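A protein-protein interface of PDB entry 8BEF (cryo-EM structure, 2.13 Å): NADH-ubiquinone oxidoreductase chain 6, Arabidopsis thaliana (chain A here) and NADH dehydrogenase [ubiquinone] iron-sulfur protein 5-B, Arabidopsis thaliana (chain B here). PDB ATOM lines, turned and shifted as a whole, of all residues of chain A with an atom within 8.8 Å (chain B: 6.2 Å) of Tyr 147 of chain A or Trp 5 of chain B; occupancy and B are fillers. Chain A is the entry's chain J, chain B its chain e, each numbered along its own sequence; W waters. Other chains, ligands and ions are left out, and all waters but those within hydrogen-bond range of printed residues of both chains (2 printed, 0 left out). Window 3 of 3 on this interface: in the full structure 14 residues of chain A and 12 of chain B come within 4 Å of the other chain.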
ATOM      1  N   TRP A 134       2.694 -26.503   7.443  1.00  0.00           N
ATOM      2  CA  TRP A 134       1.801 -26.059   8.503  1.00  0.00           C
ATOM      3  C   TRP A 134       1.817 -27.060   9.648  1.00  0.00           C
ATOM      4  O   TRP A 134       1.776 -28.272   9.425  1.00  0.00           O
ATOM      5  CB  TRP A 134       0.368 -25.904   7.987  1.00  0.00           C
ATOM      6  CG  TRP A 134       0.090 -24.607   7.298  1.00  0.00           C
ATOM      7  CD1 TRP A 134       1.004 -23.747   6.759  1.00  0.00           C
ATOM      8  CD2 TRP A 134      -1.198 -24.018   7.069  1.00  0.00           C
ATOM      9  NE1 TRP A 134       0.366 -22.659   6.212  1.00  0.00           N
ATOM     10  CE2 TRP A 134      -0.986 -22.802   6.390  1.00  0.00           C
ATOM     11  CE3 TRP A 134      -2.506 -24.400   7.379  1.00  0.00           C
ATOM     12  CZ2 TRP A 134      -2.037 -21.968   6.009  1.00  0.00           C
ATOM     13  CZ3 TRP A 134      -3.547 -23.570   7.001  1.00  0.00           C
ATOM     14  CH2 TRP A 134      -3.307 -22.370   6.322  1.00  0.00           C
ATOM     15  N   THR A 139      -3.114 -25.505  11.134  1.00  0.00           N
ATOM     16  CA  THR A 139      -4.129 -26.034  10.226  1.00  0.00           C
ATOM     17  C   THR A 139      -5.503 -26.059  10.886  1.00  0.00           C
ATOM     18  O   THR A 139      -6.506 -25.707  10.257  1.00  0.00           O
ATOM     19  CB  THR A 139      -3.738 -27.430   9.732  1.00  0.00           C
ATOM     20  OG1 THR A 139      -2.372 -27.430   9.300  1.00  0.00           O
ATOM     21  CG2 THR A 139      -4.633 -27.858   8.572  1.00  0.00           C
ATOM     22  N   LEU A 140      -5.572 -26.474  12.155  1.00  0.00           N
ATOM     23  CA  LEU A 140      -6.853 -26.459  12.862  1.00  0.00           C
ATOM     24  C   LEU A 140      -7.351 -25.032  13.098  1.00  0.00           C
ATOM     25  O   LEU A 140      -8.547 -24.738  12.926  1.00  0.00           O
ATOM     26  CB  LEU A 140      -6.717 -27.209  14.186  1.00  0.00           C
ATOM     27  CG  LEU A 140      -7.997 -27.597  14.920  1.00  0.00           C
ATOM     28  CD1 LEU A 140      -8.985 -28.252  13.970  1.00  0.00           C
ATOM     29  CD2 LEU A 140      -7.663 -28.522  16.084  1.00  0.00           C
ATOM     30  N   GLY A 141      -6.444 -24.131  13.489  1.00  0.00           N
ATOM     31  CA  GLY A 141      -6.825 -22.764  13.793  1.00  0.00           C
ATOM     32  C   GLY A 141      -7.211 -21.950  12.580  1.00  0.00           C
ATOM     33  O   GLY A 141      -7.898 -20.933  12.723  1.00  0.00           O
ATOM     34  N   ASN A 142      -6.775 -22.366  11.392  1.00  0.00           N
ATOM     35  CA  ASN A 142      -7.241 -21.753  10.157  1.00  0.00           C
ATOM     36  C   ASN A 142      -8.734 -21.969   9.927  1.00  0.00           C
ATOM     37  O   ASN A 142      -9.346 -21.221   9.158  1.00  0.00           O
ATOM     38  CB  ASN A 142      -6.438 -22.324   8.985  1.00  0.00           C
ATOM     39  CG  ASN A 142      -6.779 -21.670   7.665  1.00  0.00           C
ATOM     40  OD1 ASN A 142      -6.771 -20.447   7.543  1.00  0.00           O
ATOM     41  ND2 ASN A 142      -7.081 -22.485   6.665  1.00  0.00           N
ATOM     42  N   LEU A 143      -9.332 -22.971  10.568  1.00  0.00           N
ATOM     43  CA  LEU A 143     -10.709 -23.363  10.299  1.00  0.00           C
ATOM     44  C   LEU A 143     -11.673 -23.118  11.444  1.00  0.00           C
ATOM     45  O   LEU A 143     -12.839 -22.814  11.187  1.00  0.00           O
ATOM     46  CB  LEU A 143     -10.778 -24.850   9.940  1.00  0.00           C
ATOM     47  CG  LEU A 143      -9.966 -25.292   8.729  1.00  0.00           C
ATOM     48  CD1 LEU A 143     -10.081 -26.792   8.575  1.00  0.00           C
ATOM     49  CD2 LEU A 143     -10.452 -24.569   7.489  1.00  0.00           C
ATOM     50  N   LEU A 144     -11.227 -23.266  12.695  1.00  0.00           N
ATOM     51  CA  LEU A 144     -12.175 -23.266  13.810  1.00  0.00           C
ATOM     52  C   LEU A 144     -12.976 -21.968  13.892  1.00  0.00           C
ATOM     53  O   LEU A 144     -14.183 -21.992  14.157  1.00  0.00           O
ATOM     54  CB  LEU A 144     -11.439 -23.501  15.125  1.00  0.00           C
ATOM     55  CG  LEU A 144     -10.975 -24.930  15.392  1.00  0.00           C
ATOM     56  CD1 LEU A 144     -10.144 -24.968  16.658  1.00  0.00           C
ATOM     57  CD2 LEU A 144     -12.170 -25.866  15.484  1.00  0.00           C
ATOM     58  N   TYR A 145     -12.327 -20.829  13.680  1.00  0.00           N
ATOM     59  CA  TYR A 145     -12.896 -19.541  14.043  1.00  0.00           C
ATOM     60  C   TYR A 145     -13.496 -18.776  12.871  1.00  0.00           C
ATOM     61  O   TYR A 145     -14.102 -17.723  13.091  1.00  0.00           O
ATOM     62  CB  TYR A 145     -11.817 -18.690  14.723  1.00  0.00           C
ATOM     63  CG  TYR A 145     -11.025 -19.511  15.708  1.00  0.00           C
ATOM     64  CD1 TYR A 145     -11.569 -19.872  16.934  1.00  0.00           C
ATOM     65  CD2 TYR A 145      -9.765 -19.993  15.381  1.00  0.00           C
ATOM     66  CE1 TYR A 145     -10.859 -20.650  17.827  1.00  0.00           C
ATOM     67  CE2 TYR A 145      -9.051 -20.777  16.261  1.00  0.00           C
ATOM     68  CZ  TYR A 145      -9.600 -21.101  17.487  1.00  0.00           C
ATOM     69  OH  TYR A 145      -8.886 -21.877  18.367  1.00  0.00           O
ATOM     70  N   THR A 146     -13.321 -19.245  11.637  1.00  0.00           N
ATOM     71  CA  THR A 146     -13.878 -18.539  10.490  1.00  0.00           C
ATOM     72  C   THR A 146     -14.888 -19.370   9.711  1.00  0.00           C
ATOM     73  O   THR A 146     -16.072 -19.025   9.692  1.00  0.00           O
ATOM     74  CB  THR A 146     -12.731 -18.079   9.584  1.00  0.00           C
ATOM     75  OG1 THR A 146     -11.867 -19.188   9.312  1.00  0.00           O
ATOM     76  CG2 THR A 146     -11.931 -16.983  10.263  1.00  0.00           C
ATOM     77  N   TYR A 147     -14.477 -20.498   9.130  1.00  0.00           N
ATOM     78  CA  TYR A 147     -15.366 -21.250   8.254  1.00  0.00           C
ATOM     79  C   TYR A 147     -16.340 -22.130   9.019  1.00  0.00           C
ATOM     80  O   TYR A 147     -17.403 -22.458   8.488  1.00  0.00           O
ATOM     81  CB  TYR A 147     -14.547 -22.083   7.262  1.00  0.00           C
ATOM     82  CG  TYR A 147     -13.715 -21.213   6.353  1.00  0.00           C
ATOM     83  CD1 TYR A 147     -14.276 -20.626   5.225  1.00  0.00           C
ATOM     84  CD2 TYR A 147     -12.388 -20.933   6.646  1.00  0.00           C
ATOM     85  CE1 TYR A 147     -13.536 -19.813   4.407  1.00  0.00           C
ATOM     86  CE2 TYR A 147     -11.637 -20.118   5.830  1.00  0.00           C
ATOM     87  CZ  TYR A 147     -12.217 -19.561   4.710  1.00  0.00           C
ATOM     88  OH  TYR A 147     -11.486 -18.744   3.887  1.00  0.00           O
ATOM     89  N   TYR A 148     -16.018 -22.497  10.254  1.00  0.00           N
ATOM     90  CA  TYR A 148     -16.884 -23.347  11.059  1.00  0.00           C
ATOM     91  C   TYR A 148     -17.132 -22.722  12.427  1.00  0.00           C
ATOM     92  O   TYR A 148     -17.242 -23.417  13.438  1.00  0.00           O
ATOM     93  CB  TYR A 148     -16.287 -24.748  11.172  1.00  0.00           C
ATOM     94  CG  TYR A 148     -16.162 -25.408   9.819  1.00  0.00           C
ATOM     95  CD1 TYR A 148     -17.247 -26.046   9.239  1.00  0.00           C
ATOM     96  CD2 TYR A 148     -14.970 -25.361   9.104  1.00  0.00           C
ATOM     97  CE1 TYR A 148     -17.152 -26.632   7.996  1.00  0.00           C
ATOM     98  CE2 TYR A 148     -14.864 -25.951   7.856  1.00  0.00           C
ATOM     99  CZ  TYR A 148     -15.962 -26.584   7.309  1.00  0.00           C
ATOM    100  OH  TYR A 148     -15.875 -27.177   6.072  1.00  0.00           O
ATOM    101  N   PHE A 149     -17.266 -21.393  12.462  1.00  0.00           N
ATOM    102  CA  PHE A 149     -17.350 -20.677  13.734  1.00  0.00           C
ATOM    103  C   PHE A 149     -18.656 -20.956  14.478  1.00  0.00           C
ATOM    104  O   PHE A 149     -18.688 -20.882  15.714  1.00  0.00           O
ATOM    105  CB  PHE A 149     -17.152 -19.173  13.499  1.00  0.00           C
ATOM    106  CG  PHE A 149     -18.364 -18.465  12.953  1.00  0.00           C
ATOM    107  CD1 PHE A 149     -18.656 -18.503  11.600  1.00  0.00           C
ATOM    108  CD2 PHE A 149     -19.196 -17.740  13.791  1.00  0.00           C
ATOM    109  CE1 PHE A 149     -19.771 -17.858  11.094  1.00  0.00           C
ATOM    110  CE2 PHE A 149     -20.309 -17.088  13.292  1.00  0.00           C
ATOM    111  CZ  PHE A 149     -20.596 -17.147  11.939  1.00  0.00           C
ATOM    112  N   VAL A 150     -19.731 -21.285  13.757  1.00  0.00           N
ATOM    113  CA  VAL A 150     -21.016 -21.540  14.410  1.00  0.00           C
ATOM    114  C   VAL A 150     -20.922 -22.744  15.343  1.00  0.00           C
ATOM    115  O   VAL A 150     -21.457 -22.725  16.458  1.00  0.00           O
ATOM    116  CB  VAL A 150     -22.127 -21.720  13.359  1.00  0.00           C
ATOM    117  CG1 VAL A 150     -23.450 -22.047  14.035  1.00  0.00           C
ATOM    118  CG2 VAL A 150     -22.258 -20.466  12.511  1.00  0.00           C
ATOM    119  N   TRP A 151     -20.258 -23.815  14.898  1.00  0.00           N
ATOM    120  CA  TRP A 151     -20.106 -25.004  15.735  1.00  0.00           C
ATOM    121  C   TRP A 151     -19.270 -24.702  16.978  1.00  0.00           C
ATOM    122  O   TRP A 151     -19.573 -25.179  18.079  1.00  0.00           O
ATOM    123  CB  TRP A 151     -19.485 -26.135  14.912  1.00  0.00           C
ATOM    124  CG  TRP A 151     -20.258 -26.475  13.662  1.00  0.00           C
ATOM    125  CD1 TRP A 151     -21.542 -26.118  13.369  1.00  0.00           C
ATOM    126  CD2 TRP A 151     -19.804 -27.271  12.559  1.00  0.00           C
ATOM    127  NE1 TRP A 151     -21.910 -26.626  12.148  1.00  0.00           N
ATOM    128  CE2 TRP A 151     -20.861 -27.338  11.631  1.00  0.00           C
ATOM    129  CE3 TRP A 151     -18.605 -27.924  12.265  1.00  0.00           C
ATOM    130  CZ2 TRP A 151     -20.755 -28.035  10.430  1.00  0.00           C
ATOM    131  CZ3 TRP A 151     -18.501 -28.618  11.072  1.00  0.00           C
ATOM    132  CH2 TRP A 151     -19.572 -28.667  10.170  1.00  0.00           C
ATOM    133  N   PHE A 152     -18.212 -23.911  16.804  1.00  0.00           N
ATOM    134  CA  PHE A 152     -17.411 -23.386  17.907  1.00  0.00           C
ATOM    135  C   PHE A 152     -18.290 -22.687  18.952  1.00  0.00           C
ATOM    136  O   PHE A 152     -18.220 -22.979  20.158  1.00  0.00           O
ATOM    137  CB  PHE A 152     -16.373 -22.441  17.284  1.00  0.00           C
ATOM    138  CG  PHE A 152     -15.508 -21.698  18.252  1.00  0.00           C
ATOM    139  CD1 PHE A 152     -14.783 -22.358  19.226  1.00  0.00           C
ATOM    140  CD2 PHE A 152     -15.366 -20.322  18.132  1.00  0.00           C
ATOM    141  CE1 PHE A 152     -13.968 -21.655  20.087  1.00  0.00           C
ATOM    142  CE2 PHE A 152     -14.552 -19.617  18.995  1.00  0.00           C
ATOM    143  CZ  PHE A 152     -13.852 -20.284  19.970  1.00  0.00           C
ATOM    144  N   ALA B   2     -14.117 -35.017   0.883  1.00  0.00           N
ATOM    145  CA  ALA B   2     -14.935 -34.054   0.124  1.00  0.00           C
ATOM    146  C   ALA B   2     -14.753 -32.567   0.427  1.00  0.00           C
ATOM    147  O   ALA B   2     -15.148 -31.834  -0.367  1.00  0.00           O
ATOM    148  CB  ALA B   2     -16.370 -34.501   0.263  1.00  0.00           C
ATOM    149  N   SER B   3     -14.316 -32.224   1.642  1.00  0.00           N
ATOM    150  CA  SER B   3     -14.256 -30.803   2.073  1.00  0.00           C
ATOM    151  C   SER B   3     -13.207 -30.017   1.290  1.00  0.00           C
ATOM    152  O   SER B   3     -13.375 -28.829   1.173  1.00  0.00           O
ATOM    153  CB  SER B   3     -13.999 -30.700   3.609  1.00  0.00           C
ATOM    154  OG  SER B   3     -12.627 -30.840   3.920  1.00  0.00           O
ATOM    155  N   GLY B   4     -12.106 -30.664   0.923  1.00  0.00           N
ATOM    156  CA  GLY B   4     -10.982 -29.950   0.303  1.00  0.00           C
ATOM    157  C   GLY B   4      -9.897 -29.417   1.225  1.00  0.00           C
ATOM    158  O   GLY B   4      -8.853 -29.084   0.730  1.00  0.00           O
ATOM    159  N   TRP B   5     -10.143 -29.356   2.548  1.00  0.00           N
ATOM    160  CA  TRP B   5      -9.122 -28.876   3.476  1.00  0.00           C
ATOM    161  C   TRP B   5      -8.176 -30.026   3.814  1.00  0.00           C
ATOM    162  O   TRP B   5      -8.578 -31.002   4.455  1.00  0.00           O
ATOM    163  CB  TRP B   5      -9.765 -28.310   4.740  1.00  0.00           C
ATOM    164  CG  TRP B   5     -10.775 -27.208   4.517  1.00  0.00           C
ATOM    165  CD1 TRP B   5     -12.132 -27.328   4.541  1.00  0.00           C
ATOM    166  CD2 TRP B   5     -10.501 -25.824   4.265  1.00  0.00           C
ATOM    167  NE1 TRP B   5     -12.721 -26.111   4.316  1.00  0.00           N
ATOM    168  CE2 TRP B   5     -11.744 -25.170   4.143  1.00  0.00           C
ATOM    169  CE3 TRP B   5      -9.329 -25.075   4.134  1.00  0.00           C
ATOM    170  CZ2 TRP B   5     -11.846 -23.804   3.892  1.00  0.00           C
ATOM    171  CZ3 TRP B   5      -9.432 -23.719   3.885  1.00  0.00           C
ATOM    172  CH2 TRP B   5     -10.682 -23.096   3.767  1.00  0.00           C
ATOM    173  N   GLY B   6      -6.917 -29.912   3.389  1.00  0.00           N
ATOM    174  CA  GLY B   6      -5.940 -30.939   3.682  1.00  0.00           C
ATOM    175  C   GLY B   6      -5.324 -30.794   5.064  1.00  0.00           C
ATOM    176  O   GLY B   6      -5.299 -29.720   5.659  1.00  0.00           O
ATOM    177  N   ILE B   7      -4.800 -31.902   5.529  1.00  0.00           N
ATOM    178  CA  ILE B   7      -4.259 -31.956   6.938  1.00  0.00           C
ATOM    179  C   ILE B   7      -2.921 -31.223   7.055  1.00  0.00           C
ATOM    180  O   ILE B   7      -2.556 -30.962   8.150  1.00  0.00           O
ATOM    181  CB  ILE B   7      -4.269 -33.401   7.471  1.00  0.00           C
ATOM    182  CG1 ILE B   7      -3.277 -34.294   6.715  1.00  0.00           C
ATOM    183  CG2 ILE B   7      -5.680 -33.963   7.493  1.00  0.00           C
ATOM    184  CD1 ILE B   7      -3.043 -35.634   7.348  1.00  0.00           C
ATOM    185  N   GLY B   9      -2.415 -28.240   5.148  1.00  0.00           N
ATOM    186  CA  GLY B   9      -2.637 -26.886   4.680  1.00  0.00           C
ATOM    187  C   GLY B   9      -2.689 -26.698   3.181  1.00  0.00           C
ATOM    188  O   GLY B   9      -2.551 -25.562   2.714  1.00  0.00           O
ATOM    189  N   ASN B  10      -2.873 -27.765   2.410  1.00  0.00           N
ATOM    190  CA  ASN B  10      -3.071 -27.680   0.969  1.00  0.00           C
ATOM    191  C   ASN B  10      -4.351 -28.418   0.598  1.00  0.00           C
ATOM    192  O   ASN B  10      -5.022 -29.000   1.451  1.00  0.00           O
ATOM    193  CB  ASN B  10      -1.867 -28.246   0.205  1.00  0.00           C
ATOM    194  CG  ASN B  10      -0.676 -27.315   0.236  1.00  0.00           C
ATOM    195  OD1 ASN B  10      -0.704 -26.233  -0.346  1.00  0.00           O
ATOM    196  ND2 ASN B  10       0.374 -27.728   0.923  1.00  0.00           N
ATOM    197  N   LYS B  11      -4.693 -28.383  -0.690  1.00  0.00           N
ATOM    198  CA  LYS B  11      -5.866 -29.102  -1.169  1.00  0.00           C
ATOM    199  C   LYS B  11      -5.763 -30.579  -0.807  1.00  0.00           C
ATOM    200  O   LYS B  11      -4.703 -31.193  -0.937  1.00  0.00           O
ATOM    201  CB  LYS B  11      -6.014 -28.940  -2.686  1.00  0.00           C
ATOM    202  CG  LYS B  11      -7.099 -29.815  -3.300  1.00  0.00           C
ATOM    203  CD  LYS B  11      -6.940 -29.953  -4.812  1.00  0.00           C
ATOM    204  CE  LYS B  11      -6.998 -28.604  -5.503  1.00  0.00           C
ATOM    205  NZ  LYS B  11      -8.075 -27.748  -4.949  1.00  0.00           N
ATOM    206  N   GLY B  12      -6.852 -31.077  -0.253  1.00  0.00           N
ATOM    207  CA  GLY B  12      -6.937 -32.507   0.082  1.00  0.00           C
ATOM    208  C   GLY B  12      -6.568 -33.433  -1.080  1.00  0.00           C
ATOM    209  O   GLY B  12      -6.903 -33.054  -2.189  1.00  0.00           O
ATOM    210  N   TYR B  15      -9.820 -34.470  -3.290  1.00  0.00           N
ATOM    211  CA  TYR B  15     -10.758 -33.364  -3.573  1.00  0.00           C
ATOM    212  C   TYR B  15     -11.023 -33.136  -5.083  1.00  0.00           C
ATOM    213  O   TYR B  15     -12.148 -32.946  -5.377  1.00  0.00           O
ATOM    214  CB  TYR B  15     -10.271 -32.093  -2.888  1.00  0.00           C
ATOM    215  CG  TYR B  15     -11.202 -30.944  -3.117  1.00  0.00           C
ATOM    216  CD1 TYR B  15     -12.446 -30.927  -2.513  1.00  0.00           C
ATOM    217  CD2 TYR B  15     -10.865 -29.922  -3.981  1.00  0.00           C
ATOM    218  CE1 TYR B  15     -13.316 -29.874  -2.708  1.00  0.00           C
ATOM    219  CE2 TYR B  15     -11.719 -28.858  -4.188  1.00  0.00           C
ATOM    220  CZ  TYR B  15     -12.941 -28.840  -3.541  1.00  0.00           C
ATOM    221  OH  TYR B  15     -13.798 -27.826  -3.761  1.00  0.00           O
HETATM  222  O   HOH W   1      -0.150 -30.296   9.734  1.00  0.00           O
HETATM  223  O   HOH W   2     -15.556 -25.798   3.798  1.00  0.00           O
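Printed residues of chain B that touch a printed residue of chain A: Trp 5, Gly 6, Ile 7 and Gly 9. Hydrophobic or aromatic side chains of chain B within 4 Å of the printed part of chain A: Trp 5. Along chain B the printed residues that touch a printed residue of chain A span positions 5 to 9. Of the 15 printed residues of chain A, 6 touch a printed residue of chain B. Hydrophobic or aromatic side chains of chain A that line the printed part of chain B: Trp 134, Leu 143, Tyr 147 and Tyr 148. Among the printed residues, no Asp or Glu carboxylate lies within 4 Å of a Lys or Arg side-chain nitrogen of the other chain.
OG of Ser 3 of chain B lies within hydrogen-bond range of N of Trp 5 of chain B (3.2 Å). The backbone carbonyl oxygen of Asn 142 of chain A is in hydrogen-bond range of the side-chain hydroxyl of Thr 146 of chain A (3.2 Å). O of Leu 143 of chain A lies within hydrogen-bond range of N of Tyr 148 of chain A, 3.3 Å away.
Printed residues of chain B within 4 Å of Trp 134 of chain A: Gly 9 (3.7 Å). Of the printed residues of chain B, Thr 139 of chain A touches Gly 6 and Ile 7. Gly 141 of chain A touches none of the printed residues of chain B. Printed residues of chain B within 4 Å of Asn 142 of chain A: Trp 5. Of the printed residues of chain B, Leu 143 of chain A touches Trp 5 (3.5 Å). Of the printed residues of chain B, Tyr 147 of chain A touches Trp 5. Of the printed residues of chain B, Tyr 148 of chain A touches Trp 5 (3.8 Å). Trp 151 of chain A touches none of the printed residues of chain B. Of chain A, only Asn 142, Leu 143, Tyr 147 and Tyr 148 come within 4 Å of Trp 5 of chain B. Gly 6 of chain B touches just one residue of chain A: Thr 139 (3.5 Å). The nearest printed residue of chain B that does not touch Tyr 147 of chain A is Ser 3 of chain B (9.2 Å). The nearest printed residue of chain B that does not touch Asn 142 of chain A is Gly 9 of chain B (6.6 Å).
Water W2 lies within hydrogen-bond range of the side-chain hydroxyl of Tyr 148 of chain A (2.7 Å) and the indole nitrogen of Trp 5 of chain B (2.9 Å). Water W1 lies within hydrogen-bond range of O of Trp 134 of chain A (2.8 Å) and O of Ile 7 of chain B (3.0 Å).
Gly 9 of chain B touches Trp 134 of chain A (CA to CE3, 3.7 Å). CG2 of Thr 139 of chain A touches O of Gly 6 of chain B (3.5 Å). Thr 139 of chain A touches Ile 7 of chain B (OG1 to O, 3.7 Å). Asn 142 of chain A touches Trp 5 of chain B (ND2 to CZ3, 3.8 Å). Leu 143 of chain A touches Trp 5 of chain B. Tyr 147 of chain A touches Trp 5 of chain B. OH of Tyr 148 of chain A touches NE1 of Trp 5 of chain B (3.8 Å).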
